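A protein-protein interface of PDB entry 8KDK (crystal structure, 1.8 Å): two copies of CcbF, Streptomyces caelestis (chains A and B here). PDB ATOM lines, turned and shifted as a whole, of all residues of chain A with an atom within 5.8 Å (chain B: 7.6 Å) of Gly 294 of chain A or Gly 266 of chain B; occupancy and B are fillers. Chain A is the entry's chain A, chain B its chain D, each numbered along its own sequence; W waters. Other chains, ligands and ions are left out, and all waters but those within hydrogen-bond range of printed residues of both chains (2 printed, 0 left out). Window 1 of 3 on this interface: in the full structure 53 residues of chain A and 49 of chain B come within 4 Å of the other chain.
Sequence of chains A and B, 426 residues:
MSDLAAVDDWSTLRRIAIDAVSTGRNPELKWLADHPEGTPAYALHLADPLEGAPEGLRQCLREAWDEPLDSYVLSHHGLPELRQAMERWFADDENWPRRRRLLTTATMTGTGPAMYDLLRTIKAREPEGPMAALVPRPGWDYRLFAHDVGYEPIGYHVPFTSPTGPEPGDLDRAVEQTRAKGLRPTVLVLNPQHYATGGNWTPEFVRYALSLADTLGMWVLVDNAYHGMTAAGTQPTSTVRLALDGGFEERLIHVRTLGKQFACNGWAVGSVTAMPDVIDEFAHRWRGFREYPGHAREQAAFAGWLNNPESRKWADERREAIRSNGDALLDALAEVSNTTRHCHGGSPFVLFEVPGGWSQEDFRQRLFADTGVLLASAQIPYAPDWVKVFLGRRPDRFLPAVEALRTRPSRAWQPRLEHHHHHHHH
Water W2 lies within hydrogen-bond range of the backbone carbonyl oxygen (O) of Trp 267 of chain B (2.5 Å), a ring nitrogen (NE2) of His 295 of chain A (2.8 Å) and the backbone carbonyl oxygen (O) of Met 108 of chain B (2.9 Å).
Water W1 lies within hydrogen-bond range of O of Met 108 of chain A, NE2 of His 295 of chain B and ND1 of His 295 of chain A.
Asp 70 of chain A touches Ala 263 of chain B.
C of Cys 264 of chain B touches O of Asp 70 of chain A, 3.3 Å away.
CA of Gly 266 of chain B touches O of Ser 71 of chain A, 3.4 Å away.
CE2 of Tyr 72 of chain A touches ND2 of Asn 265 of chain B (3.5 Å).
Tyr 72 of chain A touches Gly 266 of chain B (N to N, 3.8 Å).
Gly 266 of chain B touches Gly 294 of chain A (O to C, 3.8 Å).
CE1 of His 295 of chain A touches O of Met 108 of chain B, at 3.6 Å.
His 295 of chain A touches Ala 268 of chain B (CE1 to CB, 3.5 Å).
His 295 of chain A touches Glu 298 of chain B.
Glu 298 of chain A touches His 295 of chain B.
His 295 of chain A touches Met 108 of chain B, but with the chains exchanged Met 108 of chain A does not touch His 295 of chain B (4.6 Å).
His 295 of chain B touches its own counterpart, His 295 of chain A.
His 295 of chain A touches Glu 298 of chain B, and with the chains exchanged Glu 298 of chain A touches His 295 of chain B.
Glu 298 of chain B touches its own counterpart, Glu 298 of chain A.
Gly 294 of chain A touches just one residue of chain B: Gly 266 (3.8 Å).
Gly 266 of chain B touches five residues of chain A.
Of the printed residues of chain B, Ser 71 of chain A touches Asp 48 and Gly 266.
Of the printed residues of chain A, Glu 298 of chain B touches His 295 (3.6 Å) and Glu 298 (2.5 Å).
Printed residues of chain A within 4 Å of Asn 265 of chain B: Asp 70 and Tyr 72.
Tyr 292 of chain A touches none of the printed residues of chain B.
The nearest residue of chain B that does not touch Gly 294 of chain A is Asn 265 of chain B (5.5 Å).
The nearest residue of chain A that does not touch Gly 266 of chain B is Ala 296 of chain A (4.8 Å).
The side-chain carboxylate (OE2) of Glu 298 of chain B sits close to the side-chain carboxylate (OE2) of Glu 298 of chain A, at 2.5 Å.
The backbone carbonyl oxygen of Asp 70 of chain A lies within hydrogen-bond range of the backbone NH of Asn 265 of chain B, 3.4 Å away.
OP2 of LLP 260 of chain B sits at hydrogen-bond distance from the side-chain hydroxyl of Tyr 72 of chain A.
NE2 of His 295 of chain B lies close to NE2 of His 295 of chain A (3.3 Å).
The side-chain carboxylate (OD1) of Asp 48 of chain B sits at hydrogen-bond distance from the backbone NH (N) of Tyr 72 of chain A (3.2 Å).
N of Gly 266 of chain B is in hydrogen-bond range of O of Asp 70 of chain A, 2.8 Å away.
The side-chain carboxylate (OD1) of Asp 70 of chain A sits at hydrogen-bond distance from the indole nitrogen (NE1) of Trp 267 of chain B, at 2.8 Å.
O of Gly 266 of chain B lies within hydrogen-bond range of N of His 295 of chain A (2.8 Å).
The backbone carbonyl oxygen (O) of Trp 267 of chain B is in hydrogen-bond range of a ring nitrogen (NE2) of His 295 of chain A.
OD1 of Asp 48 of chain B is in hydrogen-bond range of ND2 of Asn 265 of chain B (2.7 Å).
The side-chain amide oxygen of Asn 265 of chain B sits close to the backbone carbonyl oxygen of Gly 259 of chain B (3.3 Å).
The backbone NH (N) of Gly 294 of chain A lies within hydrogen-bond range of the side-chain sulfur (SD) of Met 108 of chain A, at 3.6 Å.
The backbone carbonyl oxygen (O) of Gly 259 of chain B sits at hydrogen-bond distance from the backbone NH (N) of Cys 264 of chain B.
N of LLP 260 of chain B lies within hydrogen-bond range of the side-chain amide oxygen of Asn 265 of chain B (3.3 Å).
O of Gly 294 of chain A lies within hydrogen-bond range of NE2 of Gln 299 of chain A, at 2.8 Å.
Of the 13 printed residues of chain A, 6 touch a printed residue of chain B.
Hydrophobic or aromatic side chains of chain A that line the printed part of chain B: Tyr 72 and His 295.
Hydrophobic or aromatic side chains of chain B that line the printed part of chain A: Trp 267, Ala 268 and His 295.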
ATOM      1  N   LEU A  69     -15.587  20.292  -4.186  1.00  0.00           N
ATOM      2  CA  LEU A  69     -16.516  19.171  -4.262  1.00  0.00           C
ATOM      3  C   LEU A  69     -15.787  17.862  -4.531  1.00  0.00           C
ATOM      4  O   LEU A  69     -16.364  16.928  -5.097  1.00  0.00           O
ATOM      5  CB  LEU A  69     -17.563  19.386  -5.350  1.00  0.00           C
ATOM      6  CG  LEU A  69     -18.598  20.457  -5.039  1.00  0.00           C
ATOM      7  CD1 LEU A  69     -19.238  20.895  -6.341  1.00  0.00           C
ATOM      8  CD2 LEU A  69     -19.616  19.903  -4.061  1.00  0.00           C
ATOM      9  N   ASP A  70     -14.529  17.778  -4.130  1.00  0.00           N
ATOM     10  CA  ASP A  70     -13.701  16.642  -4.493  1.00  0.00           C
ATOM     11  C   ASP A  70     -13.635  15.598  -3.403  1.00  0.00           C
ATOM     12  O   ASP A  70     -13.106  14.513  -3.639  1.00  0.00           O
ATOM     13  CB  ASP A  70     -12.296  17.129  -4.857  1.00  0.00           C
ATOM     14  CG  ASP A  70     -12.338  18.129  -5.991  1.00  0.00           C
ATOM     15  OD1 ASP A  70     -12.795  17.741  -7.078  1.00  0.00           O
ATOM     16  OD2 ASP A  70     -11.954  19.294  -5.788  1.00  0.00           O
ATOM     17  N   SER A  71     -14.193  15.886  -2.236  1.00  0.00           N
ATOM     18  CA  SER A  71     -13.982  15.037  -1.074  1.00  0.00           C
ATOM     19  C   SER A  71     -15.037  13.944  -0.989  1.00  0.00           C
ATOM     20  O   SER A  71     -16.004  13.891  -1.761  1.00  0.00           O
ATOM     21  CB  SER A  71     -14.007  15.873   0.199  1.00  0.00           C
ATOM     22  OG  SER A  71     -15.341  16.112   0.584  1.00  0.00           O
ATOM     23  N   TYR A  72     -14.855  13.067  -0.005  1.00  0.00           N
ATOM     24  CA  TYR A  72     -15.949  12.206   0.401  1.00  0.00           C
ATOM     25  C   TYR A  72     -17.121  13.069   0.843  1.00  0.00           C
ATOM     26  O   TYR A  72     -16.943  14.206   1.302  1.00  0.00           O
ATOM     27  CB  TYR A  72     -15.552  11.331   1.585  1.00  0.00           C
ATOM     28  CG  TYR A  72     -14.613  10.198   1.319  1.00  0.00           C
ATOM     29  CD1 TYR A  72     -14.808   9.324   0.242  1.00  0.00           C
ATOM     30  CD2 TYR A  72     -13.561   9.955   2.186  1.00  0.00           C
ATOM     31  CE1 TYR A  72     -13.943   8.246   0.030  1.00  0.00           C
ATOM     32  CE2 TYR A  72     -12.701   8.885   1.983  1.00  0.00           C
ATOM     33  CZ  TYR A  72     -12.906   8.039   0.908  1.00  0.00           C
ATOM     34  OH  TYR A  72     -12.049   6.983   0.706  1.00  0.00           O
ATOM     35  N   VAL A  73     -18.322  12.518   0.703  1.00  0.00           N
ATOM     36  CA  VAL A  73     -19.514  13.069   1.335  1.00  0.00           C
ATOM     37  C   VAL A  73     -19.662  12.411   2.703  1.00  0.00           C
ATOM     38  O   VAL A  73     -19.500  11.190   2.841  1.00  0.00           O
ATOM     39  CB  VAL A  73     -20.747  12.857   0.443  1.00  0.00           C
ATOM     40  CG1 VAL A  73     -22.022  13.296   1.145  1.00  0.00           C
ATOM     41  CG2 VAL A  73     -20.581  13.639  -0.855  1.00  0.00           C
ATOM     42  N   MET A 108     -24.820   6.228  -5.440  1.00  0.00           N
ATOM     43  CA  MET A 108     -23.654   6.822  -6.076  1.00  0.00           C
ATOM     44  C   MET A 108     -22.821   5.834  -6.874  1.00  0.00           C
ATOM     45  O   MET A 108     -21.779   6.227  -7.427  1.00  0.00           O
ATOM     46  CB  MET A 108     -22.763   7.483  -5.013  1.00  0.00           C
ATOM     47  CG  MET A 108     -23.327   8.769  -4.389  1.00  0.00           C
ATOM     48  SD  MET A 108     -22.898   8.951  -2.617  1.00  0.00           S
ATOM     49  CE  MET A 108     -24.039   7.776  -1.870  1.00  0.00           C
ATOM     50  N   TYR A 292     -17.796   4.190   0.500  1.00  0.00           N
ATOM     51  CA  TYR A 292     -17.815   5.502   1.127  1.00  0.00           C
ATOM     52  C   TYR A 292     -18.490   6.470   0.172  1.00  0.00           C
ATOM     53  O   TYR A 292     -18.182   6.435  -1.028  1.00  0.00           O
ATOM     54  CB  TYR A 292     -16.406   5.989   1.468  1.00  0.00           C
ATOM     55  CG  TYR A 292     -16.374   6.847   2.729  1.00  0.00           C
ATOM     56  CD1 TYR A 292     -17.000   8.102   2.760  1.00  0.00           C
ATOM     57  CD2 TYR A 292     -15.730   6.419   3.879  1.00  0.00           C
ATOM     58  CE1 TYR A 292     -17.002   8.889   3.924  1.00  0.00           C
ATOM     59  CE2 TYR A 292     -15.715   7.205   5.036  1.00  0.00           C
ATOM     60  CZ  TYR A 292     -16.347   8.440   5.048  1.00  0.00           C
ATOM     61  OH  TYR A 292     -16.353   9.212   6.198  1.00  0.00           O
ATOM     62  N   PRO A 293     -19.457   7.280   0.624  1.00  0.00           N
ATOM     63  CA  PRO A 293     -20.128   8.202  -0.305  1.00  0.00           C
ATOM     64  C   PRO A 293     -19.144   9.174  -0.944  1.00  0.00           C
ATOM     65  O   PRO A 293     -18.249   9.717  -0.293  1.00  0.00           O
ATOM     66  CB  PRO A 293     -21.161   8.933   0.567  1.00  0.00           C
ATOM     67  CG  PRO A 293     -21.149   8.286   1.902  1.00  0.00           C
ATOM     68  CD  PRO A 293     -20.181   7.128   1.902  1.00  0.00           C
ATOM     69  N   GLY A 294     -19.317   9.374  -2.245  1.00  0.00           N
ATOM     70  CA  GLY A 294     -18.411  10.207  -3.013  1.00  0.00           C
ATOM     71  C   GLY A 294     -19.144  10.754  -4.220  1.00  0.00           C
ATOM     72  O   GLY A 294     -20.371  10.813  -4.204  1.00  0.00           O
ATOM     73  N   HIS A 295     -18.421  11.148  -5.267  1.00  0.00           N
ATOM     74  CA  HIS A 295     -19.028  11.713  -6.473  1.00  0.00           C
ATOM     75  C   HIS A 295     -19.910  12.918  -6.157  1.00  0.00           C
ATOM     76  O   HIS A 295     -21.015  13.066  -6.691  1.00  0.00           O
ATOM     77  CB  HIS A 295     -19.766  10.641  -7.273  1.00  0.00           C
ATOM     78  CG  HIS A 295     -18.830   9.704  -7.939  1.00  0.00           C
ATOM     79  ND1 HIS A 295     -18.607   8.424  -7.480  1.00  0.00           N
ATOM     80  CD2 HIS A 295     -17.958   9.895  -8.959  1.00  0.00           C
ATOM     81  CE1 HIS A 295     -17.675   7.851  -8.219  1.00  0.00           C
ATOM     82  NE2 HIS A 295     -17.272   8.719  -9.131  1.00  0.00           N
ATOM     83  N   ALA A 296     -19.395  13.809  -5.297  1.00  0.00           N
ATOM     84  CA  ALA A 296     -20.107  15.045  -4.995  1.00  0.00           C
ATOM     85  C   ALA A 296     -20.270  15.926  -6.232  1.00  0.00           C
ATOM     86  O   ALA A 296     -21.261  16.656  -6.346  1.00  0.00           O
ATOM     87  CB  ALA A 296     -19.388  15.823  -3.889  1.00  0.00           C
ATOM     88  N   GLU A 298     -20.805  14.974  -9.490  1.00  0.00           N
ATOM     89  CA  GLU A 298     -22.005  14.524 -10.193  1.00  0.00           C
ATOM     90  C   GLU A 298     -23.269  14.922  -9.445  1.00  0.00           C
ATOM     91  O   GLU A 298     -24.283  15.310 -10.052  1.00  0.00           O
ATOM     92  CB  GLU A 298     -21.971  13.006 -10.376  1.00  0.00           C
ATOM     93  CG  GLU A 298     -21.105  12.557 -11.520  1.00  0.00           C
ATOM     94  CD  GLU A 298     -19.661  12.450 -11.137  1.00  0.00           C
ATOM     95  OE1 GLU A 298     -19.312  12.763  -9.974  1.00  0.00           O
ATOM     96  OE2 GLU A 298     -18.869  12.082 -12.027  1.00  0.00           O
ATOM     97  N   GLN A 299     -23.253  14.781  -8.125  1.00  0.00           N
ATOM     98  CA  GLN A 299     -24.480  14.995  -7.374  1.00  0.00           C
ATOM     99  C   GLN A 299     -24.845  16.471  -7.307  1.00  0.00           C
ATOM    100  O   GLN A 299     -26.028  16.819  -7.399  1.00  0.00           O
ATOM    101  CB  GLN A 299     -24.339  14.436  -5.964  1.00  0.00           C
ATOM    102  CG  GLN A 299     -24.239  12.913  -5.918  1.00  0.00           C
ATOM    103  CD  GLN A 299     -24.109  12.441  -4.497  1.00  0.00           C
ATOM    104  OE1 GLN A 299     -25.063  12.504  -3.740  1.00  0.00           O
ATOM    105  NE2 GLN A 299     -22.914  11.984  -4.125  1.00  0.00           N
ATOM    106  N   ASP B  48      -8.839  13.478   4.142  1.00  0.00           N
ATOM    107  CA  ASP B  48      -9.825  13.962   3.187  1.00  0.00           C
ATOM    108  C   ASP B  48      -9.756  15.486   3.182  1.00  0.00           C
ATOM    109  O   ASP B  48     -10.515  16.130   3.918  1.00  0.00           O
ATOM    110  CB  ASP B  48     -11.204  13.454   3.629  1.00  0.00           C
ATOM    111  CG  ASP B  48     -12.269  13.537   2.546  1.00  0.00           C
ATOM    112  OD1 ASP B  48     -11.972  13.265   1.373  1.00  0.00           O
ATOM    113  OD2 ASP B  48     -13.428  13.860   2.902  1.00  0.00           O
ATOM    114  N   MET B 108     -13.544   2.430 -10.497  1.00  0.00           N
ATOM    115  CA  MET B 108     -14.225   3.714 -10.587  1.00  0.00           C
ATOM    116  C   MET B 108     -15.209   3.956  -9.446  1.00  0.00           C
ATOM    117  O   MET B 108     -15.837   5.019  -9.417  1.00  0.00           O
ATOM    118  CB  MET B 108     -15.006   3.805 -11.914  1.00  0.00           C
ATOM    119  CG  MET B 108     -14.334   4.509 -13.090  1.00  0.00           C
ATOM    120  SD  MET B 108     -12.615   4.052 -13.383  1.00  0.00           S
ATOM    121  CE  MET B 108     -12.929   2.629 -14.415  1.00  0.00           C
ATOM    122  N   GLY B 259      -7.317   8.803  -5.046  1.00  0.00           N
ATOM    123  CA  GLY B 259      -7.954   9.822  -4.221  1.00  0.00           C
ATOM    124  C   GLY B 259      -7.109  10.341  -3.080  1.00  0.00           C
ATOM    125  O   GLY B 259      -7.017  11.550  -2.853  1.00  0.00           O
ATOM    126  N1  LLP B 260      -7.170   2.182   1.926  1.00  0.00           N
ATOM    127  C2  LLP B 260      -6.776   3.058   2.844  1.00  0.00           C
ATOM    128  C2' LLP B 260      -5.689   2.665   3.795  1.00  0.00           C
ATOM    129  C3  LLP B 260      -7.378   4.317   2.924  1.00  0.00           C
ATOM    130  O3  LLP B 260      -6.959   5.165   3.889  1.00  0.00           O
ATOM    131  C4  LLP B 260      -8.409   4.654   2.031  1.00  0.00           C
ATOM    132  C4' LLP B 260      -8.991   5.996   2.076  1.00  0.00           C
ATOM    133  C5  LLP B 260      -8.793   3.707   1.068  1.00  0.00           C
ATOM    134  C6  LLP B 260      -8.160   2.496   1.066  1.00  0.00           C
ATOM    135  C5' LLP B 260      -9.903   3.946   0.091  1.00  0.00           C
ATOM    136  OP4 LLP B 260      -9.637   5.054  -0.817  1.00  0.00           O
ATOM    137  P   LLP B 260     -10.681   5.295  -2.019  1.00  0.00           P
ATOM    138  OP1 LLP B 260     -10.148   6.592  -2.642  1.00  0.00           O
ATOM    139  OP2 LLP B 260     -12.063   5.419  -1.458  1.00  0.00           O
ATOM    140  OP3 LLP B 260     -10.517   4.083  -2.926  1.00  0.00           O
ATOM    141  N   LLP B 260      -6.484   9.445  -2.335  1.00  0.00           N
ATOM    142  CA  LLP B 260      -5.636   9.910  -1.203  1.00  0.00           C
ATOM    143  CB  LLP B 260      -5.264   8.727  -0.298  1.00  0.00           C
ATOM    144  CG  LLP B 260      -6.445   8.049   0.396  1.00  0.00           C
ATOM    145  CD  LLP B 260      -7.114   8.885   1.485  1.00  0.00           C
ATOM    146  CE  LLP B 260      -8.467   8.320   1.942  1.00  0.00           C
ATOM    147  NZ  LLP B 260      -8.318   6.987   2.532  1.00  0.00           N
ATOM    148  C   LLP B 260      -4.415  10.646  -1.776  1.00  0.00           C
ATOM    149  O   LLP B 260      -3.977  11.626  -1.144  1.00  0.00           O
ATOM    150  N   ALA B 263      -5.889  14.379  -3.271  1.00  0.00           N
ATOM    151  CA  ALA B 263      -6.874  15.184  -2.526  1.00  0.00           C
ATOM    152  C   ALA B 263      -8.254  15.174  -3.200  1.00  0.00           C
ATOM    153  O   ALA B 263      -8.930  16.195  -3.299  1.00  0.00           O
ATOM    154  CB  ALA B 263      -6.364  16.625  -2.338  1.00  0.00           C
ATOM    155  N   CYS B 264      -8.686  14.002  -3.653  1.00  0.00           N
ATOM    156  CA  CYS B 264      -9.903  13.884  -4.440  1.00  0.00           C
ATOM    157  C   CYS B 264     -10.569  12.540  -4.164  1.00  0.00           C
ATOM    158  O   CYS B 264     -10.949  11.810  -5.078  1.00  0.00           O
ATOM    159  CB  CYS B 264      -9.590  14.046  -5.929  1.00  0.00           C
ATOM    160  SG  CYS B 264      -8.361  12.886  -6.509  1.00  0.00           S
ATOM    161  N   ASN B 265     -10.722  12.211  -2.878  1.00  0.00           N
ATOM    162  CA  ASN B 265     -11.342  10.958  -2.474  1.00  0.00           C
ATOM    163  C   ASN B 265     -12.678  10.721  -3.163  1.00  0.00           C
ATOM    164  O   ASN B 265     -12.983   9.594  -3.557  1.00  0.00           O
ATOM    165  CB  ASN B 265     -11.544  10.952  -0.967  1.00  0.00           C
ATOM    166  CG  ASN B 265     -10.243  10.797  -0.209  1.00  0.00           C
ATOM    167  OD1 ASN B 265      -9.265  10.274  -0.741  1.00  0.00           O
ATOM    168  ND2 ASN B 265     -10.247  11.196   1.045  1.00  0.00           N
ATOM    169  N   GLY B 266     -13.506  11.760  -3.291  1.00  0.00           N
ATOM    170  CA  GLY B 266     -14.813  11.549  -3.921  1.00  0.00           C
ATOM    171  C   GLY B 266     -14.755  11.183  -5.398  1.00  0.00           C
ATOM    172  O   GLY B 266     -15.753  10.711  -5.949  1.00  0.00           O
ATOM    173  N   TRP B 267     -13.616  11.369  -6.054  1.00  0.00           N
ATOM    174  CA  TRP B 267     -13.547  10.973  -7.463  1.00  0.00           C
ATOM    175  C   TRP B 267     -13.585   9.455  -7.626  1.00  0.00           C
ATOM    176  O   TRP B 267     -13.985   8.953  -8.685  1.00  0.00           O
ATOM    177  CB  TRP B 267     -12.280  11.534  -8.100  1.00  0.00           C
ATOM    178  CG  TRP B 267     -12.332  12.990  -8.366  1.00  0.00           C
ATOM    179  CD1 TRP B 267     -12.768  13.971  -7.527  1.00  0.00           C
ATOM    180  CD2 TRP B 267     -11.909  13.633  -9.564  1.00  0.00           C
ATOM    181  NE1 TRP B 267     -12.633  15.206  -8.133  1.00  0.00           N
ATOM    182  CE2 TRP B 267     -12.120  15.019  -9.392  1.00  0.00           C
ATOM    183  CE3 TRP B 267     -11.373  13.167 -10.771  1.00  0.00           C
ATOM    184  CZ2 TRP B 267     -11.799  15.956 -10.382  1.00  0.00           C
ATOM    185  CZ3 TRP B 267     -11.061  14.104 -11.761  1.00  0.00           C
ATOM    186  CH2 TRP B 267     -11.279  15.479 -11.555  1.00  0.00           C
ATOM    187  N   ALA B 268     -13.140   8.717  -6.608  1.00  0.00           N
ATOM    188  CA  ALA B 268     -13.264   7.253  -6.562  1.00  0.00           C
ATOM    189  C   ALA B 268     -12.539   6.537  -7.710  1.00  0.00           C
ATOM    190  O   ALA B 268     -12.933   5.437  -8.110  1.00  0.00           O
ATOM    191  CB  ALA B 268     -14.744   6.841  -6.524  1.00  0.00           C
ATOM    192  N   VAL B 269     -11.437   7.086  -8.225  1.00  0.00           N
ATOM    193  CA  VAL B 269     -10.634   6.384  -9.225  1.00  0.00           C
ATOM    194  C   VAL B 269      -9.426   5.746  -8.543  1.00  0.00           C
ATOM    195  O   VAL B 269      -8.747   6.368  -7.700  1.00  0.00           O
ATOM    196  CB  VAL B 269     -10.195   7.326 -10.366  1.00  0.00           C
ATOM    197  CG1 VAL B 269      -9.436   6.554 -11.456  1.00  0.00           C
ATOM    198  CG2 VAL B 269     -11.416   8.066 -10.984  1.00  0.00           C
ATOM    199  N   HIS B 295     -18.104   6.832 -15.406  1.00  0.00           N
ATOM    200  CA  HIS B 295     -17.210   7.895 -14.949  1.00  0.00           C
ATOM    201  C   HIS B 295     -16.036   8.118 -15.892  1.00  0.00           C
ATOM    202  O   HIS B 295     -14.882   8.240 -15.476  1.00  0.00           O
ATOM    203  CB  HIS B 295     -16.739   7.622 -13.534  1.00  0.00           C
ATOM    204  CG  HIS B 295     -17.874   7.495 -12.580  1.00  0.00           C
ATOM    205  ND1 HIS B 295     -18.285   6.287 -12.063  1.00  0.00           N
ATOM    206  CD2 HIS B 295     -18.725   8.429 -12.097  1.00  0.00           C
ATOM    207  CE1 HIS B 295     -19.326   6.487 -11.277  1.00  0.00           C
ATOM    208  NE2 HIS B 295     -19.615   7.775 -11.284  1.00  0.00           N
ATOM    209  N   GLU B 298     -14.075  11.438 -15.059  1.00  0.00           N
ATOM    210  CA  GLU B 298     -12.978  11.315 -14.103  1.00  0.00           C
ATOM    211  C   GLU B 298     -11.793  10.593 -14.719  1.00  0.00           C
ATOM    212  O   GLU B 298     -10.640  10.934 -14.448  1.00  0.00           O
ATOM    213  CB  GLU B 298     -13.440  10.556 -12.865  1.00  0.00           C
ATOM    214  CG  GLU B 298     -14.236  11.400 -11.901  1.00  0.00           C
ATOM    215  CD  GLU B 298     -15.715  11.436 -12.221  1.00  0.00           C
ATOM    216  OE1 GLU B 298     -16.163  10.876 -13.251  1.00  0.00           O
ATOM    217  OE2 GLU B 298     -16.433  12.056 -11.441  1.00  0.00           O
HETATM  218  O   HOH W   1     -21.559   8.556  -9.179  1.00  0.00           O
HETATM  219  O   HOH W   2     -15.109   7.645 -10.526  1.00  0.00           O
